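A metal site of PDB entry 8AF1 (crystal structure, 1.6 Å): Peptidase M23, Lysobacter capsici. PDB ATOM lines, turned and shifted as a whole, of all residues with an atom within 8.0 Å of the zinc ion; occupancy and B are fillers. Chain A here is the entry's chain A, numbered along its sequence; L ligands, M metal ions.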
ATOM      1  N   GLY A  20     -13.948 -21.884  26.330  1.00  0.00           N
ATOM      2  CA  GLY A  20     -14.141 -21.645  27.750  1.00  0.00           C
ATOM      3  C   GLY A  20     -13.091 -20.713  28.335  1.00  0.00           C
ATOM      4  O   GLY A  20     -11.951 -20.641  27.875  1.00  0.00           O
ATOM      5  N   ALA A  21     -13.501 -19.972  29.374  1.00  0.00           N
ATOM      6  CA  ALA A  21     -12.581 -19.084  30.071  1.00  0.00           C
ATOM      7  C   ALA A  21     -11.428 -19.878  30.672  1.00  0.00           C
ATOM      8  O   ALA A  21     -11.586 -21.025  31.092  1.00  0.00           O
ATOM      9  CB  ALA A  21     -13.306 -18.308  31.159  1.00  0.00           C
ATOM     10  N   HIS A  22     -10.255 -19.253  30.704  1.00  0.00           N
ATOM     11  CA  HIS A  22      -9.081 -19.888  31.277  1.00  0.00           C
ATOM     12  C   HIS A  22      -8.135 -18.812  31.800  1.00  0.00           C
ATOM     13  O   HIS A  22      -8.278 -17.635  31.469  1.00  0.00           O
ATOM     14  CB  HIS A  22      -8.368 -20.813  30.266  1.00  0.00           C
ATOM     15  CG  HIS A  22      -8.119 -20.198  28.911  1.00  0.00           C
ATOM     16  ND1 HIS A  22      -9.114 -20.013  27.973  1.00  0.00           N
ATOM     17  CD2 HIS A  22      -6.966 -19.823  28.303  1.00  0.00           C
ATOM     18  CE1 HIS A  22      -8.596 -19.505  26.865  1.00  0.00           C
ATOM     19  NE2 HIS A  22      -7.286 -19.393  27.038  1.00  0.00           N
ATOM     20  N   THR A  23      -7.179 -19.228  32.630  1.00  0.00           N
ATOM     21  CA  THR A  23      -6.095 -18.350  33.018  1.00  0.00           C
ATOM     22  C   THR A  23      -5.183 -18.104  31.819  1.00  0.00           C
ATOM     23  O   THR A  23      -5.242 -18.803  30.801  1.00  0.00           O
ATOM     24  CB  THR A  23      -5.288 -18.954  34.167  1.00  0.00           C
ATOM     25  OG1 THR A  23      -4.632 -20.143  33.702  1.00  0.00           O
ATOM     26  CG2 THR A  23      -6.179 -19.279  35.368  1.00  0.00           C
ATOM     27  N   ASN A  24      -4.320 -17.103  31.945  1.00  0.00           N
ATOM     28  CA  ASN A  24      -3.450 -16.743  30.836  1.00  0.00           C
ATOM     29  C   ASN A  24      -2.579 -17.925  30.414  1.00  0.00           C
ATOM     30  O   ASN A  24      -2.328 -18.128  29.216  1.00  0.00           O
ATOM     31  CB  ASN A  24      -2.593 -15.545  31.202  1.00  0.00           C
ATOM     32  CG  ASN A  24      -1.716 -15.099  30.056  1.00  0.00           C
ATOM     33  OD1 ASN A  24      -2.200 -14.888  28.949  1.00  0.00           O
ATOM     34  ND2 ASN A  24      -0.427 -14.980  30.307  1.00  0.00           N
ATOM     35  N   THR A  25      -2.092 -18.716  31.385  1.00  0.00           N
ATOM     36  CA  THR A  25      -1.240 -19.843  31.064  1.00  0.00           C
ATOM     37  C   THR A  25      -2.009 -21.121  30.763  1.00  0.00           C
ATOM     38  O   THR A  25      -1.408 -22.116  30.328  1.00  0.00           O
ATOM     39  CB  THR A  25      -0.272 -20.127  32.210  1.00  0.00           C
ATOM     40  OG1 THR A  25      -1.025 -20.501  33.375  1.00  0.00           O
ATOM     41  CG2 THR A  25       0.516 -18.867  32.532  1.00  0.00           C
ATOM     42  N   GLY A  26      -3.314 -21.152  31.008  1.00  0.00           N
ATOM     43  CA  GLY A  26      -4.100 -22.331  30.738  1.00  0.00           C
ATOM     44  C   GLY A  26      -4.135 -23.340  31.863  1.00  0.00           C
ATOM     45  O   GLY A  26      -4.745 -24.411  31.686  1.00  0.00           O
ATOM     46  N   SER A  34      -9.063 -15.138  30.266  1.00  0.00           N
ATOM     47  CA  SER A  34      -8.731 -15.346  28.863  1.00  0.00           C
ATOM     48  C   SER A  34      -9.737 -16.235  28.174  1.00  0.00           C
ATOM     49  O   SER A  34     -10.317 -17.146  28.771  1.00  0.00           O
ATOM     50  CB  SER A  34      -7.334 -15.962  28.691  1.00  0.00           C
ATOM     51  OG  SER A  34      -6.337 -15.212  29.380  1.00  0.00           O
ATOM     52  N   LEU A  35      -9.909 -15.985  26.874  1.00  0.00           N
ATOM     53  CA  LEU A  35     -10.771 -16.743  25.975  1.00  0.00           C
ATOM     54  C   LEU A  35     -10.046 -16.956  24.646  1.00  0.00           C
ATOM     55  O   LEU A  35      -9.347 -16.058  24.186  1.00  0.00           O
ATOM     56  CB  LEU A  35     -12.097 -15.998  25.713  1.00  0.00           C
ATOM     57  CG  LEU A  35     -13.071 -15.720  26.861  1.00  0.00           C
ATOM     58  CD1 LEU A  35     -14.160 -14.722  26.429  1.00  0.00           C
ATOM     59  CD2 LEU A  35     -13.697 -17.011  27.345  1.00  0.00           C
ATOM     60  N   ASP A  36     -10.225 -18.121  24.040  1.00  0.00           N
ATOM     61  CA  ASP A  36      -9.664 -18.405  22.725  1.00  0.00           C
ATOM     62  C   ASP A  36     -10.759 -18.279  21.679  1.00  0.00           C
ATOM     63  O   ASP A  36     -11.879 -18.773  21.873  1.00  0.00           O
ATOM     64  CB  ASP A  36      -9.057 -19.809  22.667  1.00  0.00           C
ATOM     65  CG  ASP A  36      -7.885 -19.975  23.605  1.00  0.00           C
ATOM     66  OD1 ASP A  36      -7.272 -18.947  23.956  1.00  0.00           O
ATOM     67  OD2 ASP A  36      -7.576 -21.131  23.988  1.00  0.00           O
ATOM     68  N   MET A  37     -10.438 -17.658  20.562  1.00  0.00           N
ATOM     69  CA  MET A  37     -11.457 -17.287  19.587  1.00  0.00           C
ATOM     70  C   MET A  37     -10.873 -17.501  18.210  1.00  0.00           C
ATOM     71  O   MET A  37      -9.708 -17.176  17.977  1.00  0.00           O
ATOM     72  CB  MET A  37     -11.799 -15.826  19.839  1.00  0.00           C
ATOM     73  CG  MET A  37     -12.708 -15.708  21.027  1.00  0.00           C
ATOM     74  SD  MET A  37     -13.443 -14.111  21.192  1.00  0.00           S
ATOM     75  CE  MET A  37     -13.100 -13.804  22.940  1.00  0.00           C
ATOM     76  N   TYR A  81      -3.023 -12.474  21.698  1.00  0.00           N
ATOM     77  CA  TYR A  81      -1.821 -13.276  21.526  1.00  0.00           C
ATOM     78  C   TYR A  81      -2.043 -14.351  20.459  1.00  0.00           C
ATOM     79  O   TYR A  81      -3.180 -14.745  20.169  1.00  0.00           O
ATOM     80  CB  TYR A  81      -1.383 -13.885  22.877  1.00  0.00           C
ATOM     81  CG  TYR A  81      -0.048 -14.579  22.796  1.00  0.00           C
ATOM     82  CD1 TYR A  81       1.062 -13.897  22.343  1.00  0.00           C
ATOM     83  CD2 TYR A  81       0.096 -15.916  23.171  1.00  0.00           C
ATOM     84  CE1 TYR A  81       2.286 -14.505  22.252  1.00  0.00           C
ATOM     85  CE2 TYR A  81       1.331 -16.550  23.088  1.00  0.00           C
ATOM     86  CZ  TYR A  81       2.423 -15.825  22.616  1.00  0.00           C
ATOM     87  OH  TYR A  81       3.662 -16.393  22.507  1.00  0.00           O
ATOM     88  N   HIS A  82      -0.927 -14.818  19.881  1.00  0.00           N
ATOM     89  CA  HIS A  82      -0.872 -15.734  18.724  1.00  0.00           C
ATOM     90  C   HIS A  82      -1.216 -15.036  17.406  1.00  0.00           C
ATOM     91  O   HIS A  82      -1.902 -15.610  16.559  1.00  0.00           O
ATOM     92  CB  HIS A  82      -1.737 -16.998  18.890  1.00  0.00           C
ATOM     93  CG  HIS A  82      -1.581 -17.713  20.199  1.00  0.00           C
ATOM     94  ND1 HIS A  82      -0.381 -18.238  20.627  1.00  0.00           N
ATOM     95  CD2 HIS A  82      -2.514 -18.121  21.103  1.00  0.00           C
ATOM     96  CE1 HIS A  82      -0.563 -18.882  21.767  1.00  0.00           C
ATOM     97  NE2 HIS A  82      -1.843 -18.834  22.081  1.00  0.00           N
ATOM     98  N   SER A 116       1.628 -22.584  24.127  1.00  0.00           N
ATOM     99  CA  SER A 116       1.263 -23.735  23.321  1.00  0.00           C
ATOM    100  C   SER A 116      -0.012 -23.431  22.558  1.00  0.00           C
ATOM    101  O   SER A 116      -0.820 -22.590  22.976  1.00  0.00           O
ATOM    102  CB  SER A 116       1.062 -24.999  24.173  1.00  0.00           C
ATOM    103  OG  SER A 116       0.250 -24.724  25.304  1.00  0.00           O
ATOM    104  N   HIS A 121      -5.664 -19.304  16.299  1.00  0.00           N
ATOM    105  CA  HIS A 121      -6.688 -18.643  17.103  1.00  0.00           C
ATOM    106  C   HIS A 121      -6.045 -17.445  17.785  1.00  0.00           C
ATOM    107  O   HIS A 121      -4.821 -17.318  17.838  1.00  0.00           O
ATOM    108  CB  HIS A 121      -7.301 -19.591  18.149  1.00  0.00           C
ATOM    109  CG  HIS A 121      -6.364 -19.934  19.272  1.00  0.00           C
ATOM    110  ND1 HIS A 121      -5.359 -20.884  19.141  1.00  0.00           N
ATOM    111  CD2 HIS A 121      -6.304 -19.504  20.555  1.00  0.00           C
ATOM    112  CE1 HIS A 121      -4.708 -20.996  20.291  1.00  0.00           C
ATOM    113  NE2 HIS A 121      -5.265 -20.175  21.166  1.00  0.00           N
ATOM    114  N   GLU A 122      -6.893 -16.553  18.295  1.00  0.00           N
ATOM    115  CA  GLU A 122      -6.401 -15.520  19.195  1.00  0.00           C
ATOM    116  C   GLU A 122      -6.644 -15.958  20.627  1.00  0.00           C
ATOM    117  O   GLU A 122      -7.730 -16.469  20.953  1.00  0.00           O
ATOM    118  CB  GLU A 122      -7.057 -14.159  18.944  1.00  0.00           C
ATOM    119  CG  GLU A 122      -8.551 -14.156  19.138  1.00  0.00           C
ATOM    120  CD  GLU A 122      -9.143 -12.753  19.042  1.00  0.00           C
ATOM    121  OE1 GLU A 122     -10.066 -12.550  18.223  1.00  0.00           O
ATOM    122  OE2 GLU A 122      -8.682 -11.870  19.804  1.00  0.00           O
ATOM    123  N   HIS A 123      -5.640 -15.772  21.464  1.00  0.00           N
ATOM    124  CA  HIS A 123      -5.760 -15.925  22.908  1.00  0.00           C
ATOM    125  C   HIS A 123      -5.978 -14.505  23.430  1.00  0.00           C
ATOM    126  O   HIS A 123      -5.056 -13.687  23.449  1.00  0.00           O
ATOM    127  CB  HIS A 123      -4.512 -16.610  23.449  1.00  0.00           C
ATOM    128  CG  HIS A 123      -4.360 -16.525  24.936  1.00  0.00           C
ATOM    129  ND1 HIS A 123      -4.899 -17.458  25.799  1.00  0.00           N
ATOM    130  CD2 HIS A 123      -3.724 -15.620  25.711  1.00  0.00           C
ATOM    131  CE1 HIS A 123      -4.595 -17.130  27.039  1.00  0.00           C
ATOM    132  NE2 HIS A 123      -3.882 -16.013  27.020  1.00  0.00           N
ATOM    133  N   TRP A 124      -7.222 -14.195  23.799  1.00  0.00           N
ATOM    134  CA  TRP A 124      -7.620 -12.851  24.212  1.00  0.00           C
ATOM    135  C   TRP A 124      -7.712 -12.798  25.719  1.00  0.00           C
ATOM    136  O   TRP A 124      -8.176 -13.755  26.344  1.00  0.00           O
ATOM    137  CB  TRP A 124      -8.968 -12.486  23.567  1.00  0.00           C
ATOM    138  CG  TRP A 124      -9.644 -11.222  24.018  1.00  0.00           C
ATOM    139  CD1 TRP A 124      -9.577 -10.005  23.404  1.00  0.00           C
ATOM    140  CD2 TRP A 124     -10.564 -11.060  25.105  1.00  0.00           C
ATOM    141  NE1 TRP A 124     -10.376  -9.087  24.065  1.00  0.00           N
ATOM    142  CE2 TRP A 124     -10.999  -9.715  25.103  1.00  0.00           C
ATOM    143  CE3 TRP A 124     -11.071 -11.928  26.085  1.00  0.00           C
ATOM    144  CZ2 TRP A 124     -11.891  -9.206  26.061  1.00  0.00           C
ATOM    145  CZ3 TRP A 124     -11.974 -11.419  27.035  1.00  0.00           C
ATOM    146  CH2 TRP A 124     -12.365 -10.079  27.008  1.00  0.00           C
ATOM    147  N   SER A 125      -7.250 -11.693  26.317  1.00  0.00           N
ATOM    148  CA  SER A 125      -7.319 -11.546  27.764  1.00  0.00           C
ATOM    149  C   SER A 125      -7.775 -10.163  28.176  1.00  0.00           C
ATOM    150  O   SER A 125      -7.474  -9.154  27.525  1.00  0.00           O
ATOM    151  CB  SER A 125      -5.953 -11.818  28.429  1.00  0.00           C
ATOM    152  OG  SER A 125      -5.383 -13.032  27.971  1.00  0.00           O
ATOM    153  N   TYR A 152     -10.466 -23.635  30.835  1.00  0.00           N
ATOM    154  CA  TYR A 152     -11.050 -24.177  29.612  1.00  0.00           C
ATOM    155  C   TYR A 152     -12.364 -24.910  29.835  1.00  0.00           C
ATOM    156  O   TYR A 152     -12.942 -25.414  28.859  1.00  0.00           O
ATOM    157  CB  TYR A 152     -10.075 -25.112  28.864  1.00  0.00           C
ATOM    158  CG  TYR A 152      -8.753 -24.465  28.503  1.00  0.00           C
ATOM    159  CD1 TYR A 152      -8.667 -23.491  27.508  1.00  0.00           C
ATOM    160  CD2 TYR A 152      -7.572 -24.841  29.161  1.00  0.00           C
ATOM    161  CE1 TYR A 152      -7.450 -22.902  27.178  1.00  0.00           C
ATOM    162  CE2 TYR A 152      -6.362 -24.260  28.839  1.00  0.00           C
ATOM    163  CZ  TYR A 152      -6.304 -23.297  27.845  1.00  0.00           C
ATOM    164  OH  TYR A 152      -5.084 -22.738  27.545  1.00  0.00           O
HETATM  165  C1  LIG L   1      -4.213 -20.852  24.836  1.00  0.00           C
HETATM  166  O1  LIG L   1      -4.372 -20.098  23.869  1.00  0.00           O
HETATM  167  O2  LIG L   1      -4.787 -20.744  25.926  1.00  0.00           O
HETATM  168 ZN    ZN M   1      -5.954 -19.156  25.445  1.00  0.00          ZN
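Three residues have an atom within 4 Å of the zinc ion: His 22, Asp 36 and His 123. The nearest printed residue that does not touch the zinc ion is Tyr 152 (4.2 Å).
A ring nitrogen (ND1) of His 22 is in hydrogen-bond range of the backbone carbonyl oxygen (O) of Gly 20 (2.9 Å). The backbone carbonyl oxygen of His 123 is in hydrogen-bond range of the backbone NH of Tyr 81 (2.9 Å). N of His 22 sits at hydrogen-bond distance from O of Ser 34. The side-chain hydroxyl of Ser 125 lies within hydrogen-bond range of a ring nitrogen (NE2) of His 123 (3.5 Å). OG of Ser 34 sits close to NE2 of His 123 (3.5 Å). OD1 of Asn 24 sits at hydrogen-bond distance from NE2 of His 123 (2.8 Å).
The zinc ion is bound by the side-chain carboxylate (OD1) of Asp 36 (2.0 Å), an oxygen (O2) of the ligand (2.0 Å), a ring nitrogen (ND1) of His 123 (2.0 Å), a ring nitrogen (NE2) of His 22 (2.1 Å) and an oxygen (O1) of the ligand (2.4 Å).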
